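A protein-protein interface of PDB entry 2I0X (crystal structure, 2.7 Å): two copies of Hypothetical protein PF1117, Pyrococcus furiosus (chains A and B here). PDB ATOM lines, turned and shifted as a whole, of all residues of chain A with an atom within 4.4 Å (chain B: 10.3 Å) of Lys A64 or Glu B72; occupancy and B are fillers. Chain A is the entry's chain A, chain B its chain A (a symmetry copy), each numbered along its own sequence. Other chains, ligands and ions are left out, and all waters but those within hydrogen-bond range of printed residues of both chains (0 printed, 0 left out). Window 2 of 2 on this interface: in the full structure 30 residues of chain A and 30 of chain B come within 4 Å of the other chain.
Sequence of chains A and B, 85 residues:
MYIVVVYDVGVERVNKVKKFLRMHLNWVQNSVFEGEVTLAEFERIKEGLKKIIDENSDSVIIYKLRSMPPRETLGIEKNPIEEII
The backbone NH (N) of Ile A62 is in hydrogen-bond range of the backbone carbonyl oxygen (O) of Glu B72.
O of Pro B70 sits at hydrogen-bond distance from N of Lys A64, 2.9 Å away.
The side-chain amino group (NZ) of Lys A64 is in salt-bridge range of the side-chain carboxylate (OE1) of Glu B72.
The backbone NH (N) of Leu B74 lies within hydrogen-bond range of the backbone carbonyl oxygen (O) of Val A60 (2.8 Å).
The side-chain hydroxyl (OH) of Tyr A63 sits at hydrogen-bond distance from the side-chain carboxylate (OE1) of Glu B34, 3.2 Å away.
The backbone carbonyl oxygen (O) of Pro B69 is in hydrogen-bond range of the guanidinium group (NH1) of Arg B71 (2.6 Å).
The backbone NH (N) of Leu A65 lies within hydrogen-bond range of the backbone carbonyl oxygen (O) of Tyr A2 (2.7 Å).
The side-chain carboxylate of Glu B34 lies within salt-bridge range of the guanidinium group of Arg B71 (2.8 Å).
Among the printed residues, pairs that only touch across the chains: Phe A42 with Glu B72, Val A60 with Glu B72, Val A60 with Thr B73, Ile A61 with Val B28, Ile A61 with Gln B29, Ile A61 with Glu B72, Ile A62 with Arg B71, Tyr A63 with Val B4, Tyr A63 with Val B28, Tyr A63 with Pro B69, Tyr A63 with Pro B70, Tyr A63 with Arg B71 and Leu A65 with Pro B69.
Printed residues of chain B within 4 Å of Phe A42: Glu B72.
Printed residues of chain B within 4 Å of Val A60: Glu B72 (3.8 Å), Thr B73 (3.3 Å) and Leu B74 (2.8 Å).
Of chain B, only Arg B71 (3.4 Å) and Glu B72 (2.8 Å) come within 4 Å of Ile A62.
Lys A64 touches just these residues of chain B: Pro B70 and Glu B72.
Of the printed residues of chain A, Pro B69 touches Tyr A63 and Leu A65.
Glu B72 touches just these residues of chain A: Phe A42 (3.2 Å), Val A60 (3.8 Å), Ile A61 (3.7 Å), Ile A62 (2.8 Å) and Lys A64 (3.1 Å).
Of the printed residues of chain A, Leu B74 touches Val A60.
The nearest printed residue of chain A that does not touch Glu B72 is Tyr A63 (4.9 Å).
Hydrophobic or aromatic side chains of chain A within 4 Å of the printed part of chain B: Phe A42, Val A60, Ile A61, Ile A62, Tyr A63 and Leu A65.
Among the printed residues, 18 pairs touch across the chains.
Among the printed residues, Asp or Glu carboxylates within 4 Å of a Lys or Arg side-chain nitrogen of the other chain: Lys A64 with Glu B72.
1 position is printed for both chains.
Of the 18 pairs that touch across the chains among the printed residues, none has its exchanged pair printed and touching as well.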
ATOM      1  N   MET A   1       4.937  -3.401 -18.405  1.00  0.00           N
ATOM      2  CA  MET A   1       6.168  -2.564 -18.440  1.00  0.00           C
ATOM      3  C   MET A   1       7.293  -3.234 -17.691  1.00  0.00           C
ATOM      4  O   MET A   1       7.092  -3.885 -16.660  1.00  0.00           O
ATOM      5  CB  MET A   1       5.935  -1.190 -17.827  1.00  0.00           C
ATOM      6  CG  MET A   1       7.094  -0.224 -18.037  1.00  0.00           C
ATOM      7  SD  MET A   1       7.486  -0.006 -19.815  1.00  0.00           S
ATOM      8  CE  MET A   1       6.512   1.531 -20.317  1.00  0.00           C
ATOM      9  N   TYR A   2       8.488  -3.048 -18.223  1.00  0.00           N
ATOM     10  CA  TYR A   2       9.681  -3.633 -17.664  1.00  0.00           C
ATOM     11  C   TYR A   2      10.752  -2.582 -17.800  1.00  0.00           C
ATOM     12  O   TYR A   2      10.912  -2.003 -18.872  1.00  0.00           O
ATOM     13  CB  TYR A   2      10.064  -4.856 -18.473  1.00  0.00           C
ATOM     14  CG  TYR A   2      11.148  -5.646 -17.825  1.00  0.00           C
ATOM     15  CD1 TYR A   2      10.849  -6.779 -17.102  1.00  0.00           C
ATOM     16  CD2 TYR A   2      12.482  -5.248 -17.906  1.00  0.00           C
ATOM     17  CE1 TYR A   2      11.835  -7.501 -16.480  1.00  0.00           C
ATOM     18  CE2 TYR A   2      13.480  -5.980 -17.274  1.00  0.00           C
ATOM     19  CZ  TYR A   2      13.138  -7.104 -16.563  1.00  0.00           C
ATOM     20  OH  TYR A   2      14.082  -7.849 -15.918  1.00  0.00           O
ATOM     21  N   ILE A   3      11.489  -2.313 -16.733  1.00  0.00           N
ATOM     22  CA  ILE A   3      12.522  -1.298 -16.836  1.00  0.00           C
ATOM     23  C   ILE A   3      13.859  -1.750 -16.301  1.00  0.00           C
ATOM     24  O   ILE A   3      13.939  -2.621 -15.439  1.00  0.00           O
ATOM     25  CB  ILE A   3      12.128  -0.002 -16.108  1.00  0.00           C
ATOM     26  CG1 ILE A   3      12.212  -0.199 -14.587  1.00  0.00           C
ATOM     27  CG2 ILE A   3      10.744   0.445 -16.565  1.00  0.00           C
ATOM     28  CD1 ILE A   3      11.395  -1.360 -14.052  1.00  0.00           C
ATOM     29  N   PHE A  42       6.086   2.352 -11.014  1.00  0.00           N
ATOM     30  CA  PHE A  42       7.123   2.993 -11.802  1.00  0.00           C
ATOM     31  C   PHE A  42       7.251   4.432 -11.335  1.00  0.00           C
ATOM     32  O   PHE A  42       8.355   4.972 -11.227  1.00  0.00           O
ATOM     33  CB  PHE A  42       6.760   2.981 -13.285  1.00  0.00           C
ATOM     34  CG  PHE A  42       7.779   3.663 -14.163  1.00  0.00           C
ATOM     35  CD1 PHE A  42       8.971   3.027 -14.496  1.00  0.00           C
ATOM     36  CD2 PHE A  42       7.536   4.935 -14.673  1.00  0.00           C
ATOM     37  CE1 PHE A  42       9.904   3.649 -15.328  1.00  0.00           C
ATOM     38  CE2 PHE A  42       8.464   5.562 -15.505  1.00  0.00           C
ATOM     39  CZ  PHE A  42       9.647   4.918 -15.834  1.00  0.00           C
ATOM     40  N   VAL A  60      20.721   9.213 -13.180  1.00  0.00           N
ATOM     41  CA  VAL A  60      19.958   7.967 -13.198  1.00  0.00           C
ATOM     42  C   VAL A  60      19.211   7.796 -14.510  1.00  0.00           C
ATOM     43  O   VAL A  60      18.443   8.671 -14.901  1.00  0.00           O
ATOM     44  CB  VAL A  60      18.928   7.894 -12.050  1.00  0.00           C
ATOM     45  CG1 VAL A  60      18.154   6.588 -12.138  1.00  0.00           C
ATOM     46  CG2 VAL A  60      19.633   7.993 -10.696  1.00  0.00           C
ATOM     47  N   ILE A  61      19.452   6.677 -15.196  1.00  0.00           N
ATOM     48  CA  ILE A  61      18.772   6.379 -16.460  1.00  0.00           C
ATOM     49  C   ILE A  61      17.817   5.221 -16.242  1.00  0.00           C
ATOM     50  O   ILE A  61      18.180   4.177 -15.664  1.00  0.00           O
ATOM     51  CB  ILE A  61      19.745   5.962 -17.605  1.00  0.00           C
ATOM     52  CG1 ILE A  61      20.779   7.067 -17.854  1.00  0.00           C
ATOM     53  CG2 ILE A  61      18.961   5.723 -18.902  1.00  0.00           C
ATOM     54  CD1 ILE A  61      21.820   6.713 -18.875  1.00  0.00           C
ATOM     55  N   ILE A  62      16.587   5.410 -16.706  1.00  0.00           N
ATOM     56  CA  ILE A  62      15.560   4.376 -16.593  1.00  0.00           C
ATOM     57  C   ILE A  62      14.946   4.034 -17.945  1.00  0.00           C
ATOM     58  O   ILE A  62      14.026   4.708 -18.409  1.00  0.00           O
ATOM     59  CB  ILE A  62      14.433   4.793 -15.643  1.00  0.00           C
ATOM     60  CG1 ILE A  62      15.011   5.040 -14.236  1.00  0.00           C
ATOM     61  CG2 ILE A  62      13.374   3.693 -15.604  1.00  0.00           C
ATOM     62  CD1 ILE A  62      14.007   5.581 -13.219  1.00  0.00           C
ATOM     63  N   TYR A  63      15.470   2.987 -18.571  1.00  0.00           N
ATOM     64  CA  TYR A  63      14.957   2.535 -19.853  1.00  0.00           C
ATOM     65  C   TYR A  63      13.592   1.902 -19.661  1.00  0.00           C
ATOM     66  O   TYR A  63      13.394   1.122 -18.732  1.00  0.00           O
ATOM     67  CB  TYR A  63      15.887   1.508 -20.463  1.00  0.00           C
ATOM     68  CG  TYR A  63      17.252   2.054 -20.756  1.00  0.00           C
ATOM     69  CD1 TYR A  63      18.313   1.873 -19.855  1.00  0.00           C
ATOM     70  CD2 TYR A  63      17.502   2.720 -21.954  1.00  0.00           C
ATOM     71  CE1 TYR A  63      19.587   2.331 -20.156  1.00  0.00           C
ATOM     72  CE2 TYR A  63      18.770   3.182 -22.259  1.00  0.00           C
ATOM     73  CZ  TYR A  63      19.804   2.979 -21.369  1.00  0.00           C
ATOM     74  OH  TYR A  63      21.065   3.359 -21.728  1.00  0.00           O
ATOM     75  N   LYS A  64      12.662   2.220 -20.550  1.00  0.00           N
ATOM     76  CA  LYS A  64      11.309   1.690 -20.455  1.00  0.00           C
ATOM     77  C   LYS A  64      11.011   0.672 -21.557  1.00  0.00           C
ATOM     78  O   LYS A  64      10.715   1.036 -22.694  1.00  0.00           O
ATOM     79  CB  LYS A  64      10.329   2.860 -20.501  1.00  0.00           C
ATOM     80  CG  LYS A  64      10.579   3.862 -19.371  1.00  0.00           C
ATOM     81  CD  LYS A  64      10.069   5.255 -19.688  1.00  0.00           C
ATOM     82  CE  LYS A  64       8.563   5.313 -19.843  1.00  0.00           C
ATOM     83  NZ  LYS A  64       8.135   6.707 -20.152  1.00  0.00           N
ATOM     84  N   LEU A  65      11.089  -0.606 -21.213  1.00  0.00           N
ATOM     85  CA  LEU A  65      10.848  -1.680 -22.175  1.00  0.00           C
ATOM     86  C   LEU A  65       9.485  -2.350 -22.014  1.00  0.00           C
ATOM     87  O   LEU A  65       8.804  -2.181 -21.001  1.00  0.00           O
ATOM     88  CB  LEU A  65      11.932  -2.736 -22.021  1.00  0.00           C
ATOM     89  CG  LEU A  65      13.344  -2.161 -22.020  1.00  0.00           C
ATOM     90  CD1 LEU A  65      14.328  -3.272 -21.753  1.00  0.00           C
ATOM     91  CD2 LEU A  65      13.625  -1.479 -23.358  1.00  0.00           C
ATOM     92  N   VAL B   4      22.479  -1.809 -25.322  1.00  0.00           N
ATOM     93  CA  VAL B   4      22.852  -0.939 -24.222  1.00  0.00           C
ATOM     94  C   VAL B   4      23.850  -1.786 -23.468  1.00  0.00           C
ATOM     95  O   VAL B   4      23.527  -2.876 -23.011  1.00  0.00           O
ATOM     96  CB  VAL B   4      21.660  -0.621 -23.283  1.00  0.00           C
ATOM     97  CG1 VAL B   4      20.657   0.313 -23.960  1.00  0.00           C
ATOM     98  CG2 VAL B   4      20.978  -1.892 -22.904  1.00  0.00           C
ATOM     99  N   VAL B  28      26.378   7.179 -22.621  1.00  0.00           N
ATOM    100  CA  VAL B  28      25.196   7.773 -21.976  1.00  0.00           C
ATOM    101  C   VAL B  28      25.518   8.339 -20.598  1.00  0.00           C
ATOM    102  O   VAL B  28      25.176   9.474 -20.290  1.00  0.00           O
ATOM    103  CB  VAL B  28      24.081   6.754 -21.760  1.00  0.00           C
ATOM    104  CG1 VAL B  28      22.750   7.432 -21.949  1.00  0.00           C
ATOM    105  CG2 VAL B  28      24.268   5.560 -22.664  1.00  0.00           C
ATOM    106  N   GLN B  29      26.117   7.510 -19.755  1.00  0.00           N
ATOM    107  CA  GLN B  29      26.531   7.926 -18.430  1.00  0.00           C
ATOM    108  C   GLN B  29      27.716   7.050 -18.125  1.00  0.00           C
ATOM    109  O   GLN B  29      28.120   6.245 -18.962  1.00  0.00           O
ATOM    110  CB  GLN B  29      25.429   7.752 -17.355  1.00  0.00           C
ATOM    111  CG  GLN B  29      25.098   6.318 -16.944  1.00  0.00           C
ATOM    112  CD  GLN B  29      24.218   6.216 -15.670  1.00  0.00           C
ATOM    113  OE1 GLN B  29      23.182   6.890 -15.545  1.00  0.00           O
ATOM    114  NE2 GLN B  29      24.627   5.344 -14.737  1.00  0.00           N
ATOM    115  N   GLU B  34      25.456   2.917 -25.461  1.00  0.00           N
ATOM    116  CA  GLU B  34      24.378   2.339 -26.256  1.00  0.00           C
ATOM    117  C   GLU B  34      24.523   2.820 -27.679  1.00  0.00           C
ATOM    118  O   GLU B  34      25.162   3.838 -27.927  1.00  0.00           O
ATOM    119  CB  GLU B  34      22.993   2.745 -25.714  1.00  0.00           C
ATOM    120  CG  GLU B  34      22.755   4.234 -25.659  1.00  0.00           C
ATOM    121  CD  GLU B  34      21.319   4.635 -25.249  1.00  0.00           C
ATOM    122  OE1 GLU B  34      21.135   5.319 -24.211  1.00  0.00           O
ATOM    123  OE2 GLU B  34      20.368   4.287 -25.984  1.00  0.00           O
ATOM    124  N   LEU B  65      18.401  -5.098 -27.841  1.00  0.00           N
ATOM    125  CA  LEU B  65      17.097  -4.557 -28.222  1.00  0.00           C
ATOM    126  C   LEU B  65      16.909  -4.422 -29.732  1.00  0.00           C
ATOM    127  O   LEU B  65      17.865  -4.496 -30.505  1.00  0.00           O
ATOM    128  CB  LEU B  65      16.924  -3.186 -27.584  1.00  0.00           C
ATOM    129  CG  LEU B  65      17.231  -3.169 -26.092  1.00  0.00           C
ATOM    130  CD1 LEU B  65      17.136  -1.752 -25.586  1.00  0.00           C
ATOM    131  CD2 LEU B  65      16.259  -4.089 -25.353  1.00  0.00           C
ATOM    132  N   SER B  67      15.489  -1.648 -31.136  1.00  0.00           N
ATOM    133  CA  SER B  67      15.628  -0.235 -31.484  1.00  0.00           C
ATOM    134  C   SER B  67      15.871   0.651 -30.247  1.00  0.00           C
ATOM    135  O   SER B  67      15.691   0.199 -29.130  1.00  0.00           O
ATOM    136  CB  SER B  67      14.375   0.220 -32.225  1.00  0.00           C
ATOM    137  OG  SER B  67      13.241   0.154 -31.386  1.00  0.00           O
ATOM    138  N   MET B  68      16.273   1.904 -30.438  1.00  0.00           N
ATOM    139  CA  MET B  68      16.536   2.777 -29.296  1.00  0.00           C
ATOM    140  C   MET B  68      15.316   2.880 -28.366  1.00  0.00           C
ATOM    141  O   MET B  68      14.285   3.465 -28.725  1.00  0.00           O
ATOM    142  CB  MET B  68      16.991   4.173 -29.778  1.00  0.00           C
ATOM    143  CG  MET B  68      17.349   5.157 -28.664  1.00  0.00           C
ATOM    144  SD  MET B  68      17.934   6.767 -29.231  1.00  0.00           S
ATOM    145  CE  MET B  68      16.559   7.319 -30.129  1.00  0.00           C
ATOM    146  N   PRO B  69      15.428   2.315 -27.148  1.00  0.00           N
ATOM    147  CA  PRO B  69      14.347   2.327 -26.158  1.00  0.00           C
ATOM    148  C   PRO B  69      14.063   3.681 -25.568  1.00  0.00           C
ATOM    149  O   PRO B  69      14.922   4.552 -25.526  1.00  0.00           O
ATOM    150  CB  PRO B  69      14.848   1.366 -25.095  1.00  0.00           C
ATOM    151  CG  PRO B  69      16.319   1.649 -25.103  1.00  0.00           C
ATOM    152  CD  PRO B  69      16.627   1.660 -26.589  1.00  0.00           C
ATOM    153  N   PRO B  70      12.825   3.891 -25.127  1.00  0.00           N
ATOM    154  CA  PRO B  70      12.538   5.196 -24.539  1.00  0.00           C
ATOM    155  C   PRO B  70      13.211   5.183 -23.149  1.00  0.00           C
ATOM    156  O   PRO B  70      13.495   4.112 -22.597  1.00  0.00           O
ATOM    157  CB  PRO B  70      11.009   5.206 -24.482  1.00  0.00           C
ATOM    158  CG  PRO B  70      10.623   4.264 -25.640  1.00  0.00           C
ATOM    159  CD  PRO B  70      11.586   3.154 -25.423  1.00  0.00           C
ATOM    160  N   ARG B  71      13.488   6.354 -22.591  1.00  0.00           N
ATOM    161  CA  ARG B  71      14.147   6.424 -21.295  1.00  0.00           C
ATOM    162  C   ARG B  71      13.662   7.613 -20.482  1.00  0.00           C
ATOM    163  O   ARG B  71      13.140   8.577 -21.020  1.00  0.00           O
ATOM    164  CB  ARG B  71      15.672   6.518 -21.481  1.00  0.00           C
ATOM    165  CG  ARG B  71      16.110   7.769 -22.195  1.00  0.00           C
ATOM    166  CD  ARG B  71      17.616   7.835 -22.454  1.00  0.00           C
ATOM    167  NE  ARG B  71      18.112   6.781 -23.347  1.00  0.00           N
ATOM    168  CZ  ARG B  71      17.389   6.224 -24.304  1.00  0.00           C
ATOM    169  NH1 ARG B  71      16.130   6.608 -24.500  1.00  0.00           N
ATOM    170  NH2 ARG B  71      17.928   5.285 -25.054  1.00  0.00           N
ATOM    171  N   GLU B  72      13.839   7.528 -19.175  1.00  0.00           N
ATOM    172  CA  GLU B  72      13.444   8.590 -18.268  1.00  0.00           C
ATOM    173  C   GLU B  72      14.757   8.834 -17.522  1.00  0.00           C
ATOM    174  O   GLU B  72      15.346   7.902 -16.968  1.00  0.00           O
ATOM    175  CB  GLU B  72      12.347   8.076 -17.323  1.00  0.00           C
ATOM    176  CG  GLU B  72      11.347   9.108 -16.816  1.00  0.00           C
ATOM    177  CD  GLU B  72       9.951   8.933 -17.424  1.00  0.00           C
ATOM    178  OE1 GLU B  72       9.460   7.783 -17.513  1.00  0.00           O
ATOM    179  OE2 GLU B  72       9.332   9.955 -17.801  1.00  0.00           O
ATOM    180  N   THR B  73      15.238  10.072 -17.533  1.00  0.00           N
ATOM    181  CA  THR B  73      16.498  10.375 -16.873  1.00  0.00           C
ATOM    182  C   THR B  73      16.339  11.381 -15.756  1.00  0.00           C
ATOM    183  O   THR B  73      15.636  12.382 -15.887  1.00  0.00           O
ATOM    184  CB  THR B  73      17.529  10.933 -17.859  1.00  0.00           C
ATOM    185  OG1 THR B  73      17.116  12.235 -18.292  1.00  0.00           O
ATOM    186  CG2 THR B  73      17.654  10.020 -19.065  1.00  0.00           C
ATOM    187  N   LEU B  74      17.008  11.093 -14.650  1.00  0.00           N
ATOM    188  CA  LEU B  74      16.986  11.955 -13.487  1.00  0.00           C
ATOM    189  C   LEU B  74      18.388  12.530 -13.334  1.00  0.00           C
ATOM    190  O   LEU B  74      19.365  11.989 -13.880  1.00  0.00           O
ATOM    191  CB  LEU B  74      16.616  11.151 -12.240  1.00  0.00           C
ATOM    192  CG  LEU B  74      15.319  10.336 -12.266  1.00  0.00           C
ATOM    193  CD1 LEU B  74      15.111   9.680 -10.912  1.00  0.00           C
ATOM    194  CD2 LEU B  74      14.140  11.233 -12.603  1.00  0.00           C
ATOM    195  N   GLY B  75      18.482  13.631 -12.594  1.00  0.00           N
ATOM    196  CA  GLY B  75      19.769  14.261 -12.371  1.00  0.00           C
ATOM    197  C   GLY B  75      20.386  14.785 -13.652  1.00  0.00           C
ATOM    198  O   GLY B  75      19.753  14.803 -14.709  1.00  0.00           O
ATOM    199  N   ILE B  76      21.634  15.216 -13.548  1.00  0.00           N
ATOM    200  CA  ILE B  76      22.356  15.753 -14.688  1.00  0.00           C
ATOM    201  C   ILE B  76      22.456  14.760 -15.841  1.00  0.00           C
ATOM    202  O   ILE B  76      23.154  13.746 -15.744  1.00  0.00           O
ATOM    203  CB  ILE B  76      23.776  16.191 -14.279  1.00  0.00           C
ATOM    204  CG1 ILE B  76      24.403  15.128 -13.369  1.00  0.00           C
ATOM    205  CG2 ILE B  76      23.713  17.551 -13.595  1.00  0.00           C
ATOM    206  CD1 ILE B  76      25.865  15.365 -13.024  1.00  0.00           C
ATOM    207  N   GLU B  77      21.748  15.051 -16.932  1.00  0.00           N
ATOM    208  CA  GLU B  77      21.788  14.184 -18.100  1.00  0.00           C
ATOM    209  C   GLU B  77      23.211  14.164 -18.623  1.00  0.00           C
ATOM    210  O   GLU B  77      23.674  15.116 -19.256  1.00  0.00           O
ATOM    211  CB  GLU B  77      20.854  14.685 -19.203  1.00  0.00           C
ATOM    212  CG  GLU B  77      19.388  14.480 -18.910  1.00  0.00           C
ATOM    213  CD  GLU B  77      18.530  14.614 -20.154  1.00  0.00           C
ATOM    214  OE1 GLU B  77      18.740  13.826 -21.106  1.00  0.00           O
ATOM    215  OE2 GLU B  77      17.646  15.503 -20.176  1.00  0.00           O
ATOM    216  N   LYS B  78      23.901  13.066 -18.347  1.00  0.00           N
ATOM    217  CA  LYS B  78      25.280  12.892 -18.770  1.00  0.00           C
ATOM    218  C   LYS B  78      25.460  13.127 -20.270  1.00  0.00           C
ATOM    219  O   LYS B  78      26.590  13.220 -20.751  1.00  0.00           O
ATOM    220  CB  LYS B  78      25.749  11.481 -18.393  1.00  0.00           C
ATOM    221  CG  LYS B  78      25.490  11.102 -16.927  1.00  0.00           C
ATOM    222  CD  LYS B  78      26.420  11.829 -15.944  1.00  0.00           C
ATOM    223  CE  LYS B  78      27.794  11.170 -15.865  1.00  0.00           C
ATOM    224  NZ  LYS B  78      27.741   9.778 -15.319  1.00  0.00           N
ATOM    225  N   ASN B  79      24.348  13.228 -21.000  1.00  0.00           N
ATOM    226  CA  ASN B  79      24.391  13.441 -22.454  1.00  0.00           C
ATOM    227  C   ASN B  79      22.990  13.631 -23.066  1.00  0.00           C
ATOM    228  O   ASN B  79      22.132  12.760 -22.950  1.00  0.00           O
ATOM    229  CB  ASN B  79      25.083  12.244 -23.123  1.00  0.00           C
ATOM    230  CG  ASN B  79      25.463  12.511 -24.567  1.00  0.00           C
ATOM    231  OD1 ASN B  79      24.612  12.813 -25.402  1.00  0.00           O
ATOM    232  ND2 ASN B  79      26.748  12.397 -24.867  1.00  0.00           N
ATOM    233  N   ILE B  81      19.830  13.591 -25.339  1.00  0.00           N
ATOM    234  CA  ILE B  81      19.326  12.575 -26.264  1.00  0.00           C
ATOM    235  C   ILE B  81      19.610  12.927 -27.727  1.00  0.00           C
ATOM    236  O   ILE B  81      19.928  12.060 -28.540  1.00  0.00           O
ATOM    237  CB  ILE B  81      17.797  12.388 -26.106  1.00  0.00           C
ATOM    238  CG1 ILE B  81      17.402  12.441 -24.623  1.00  0.00           C
ATOM    239  CG2 ILE B  81      17.369  11.069 -26.737  1.00  0.00           C
ATOM    240  CD1 ILE B  81      18.007  11.355 -23.753  1.00  0.00           C
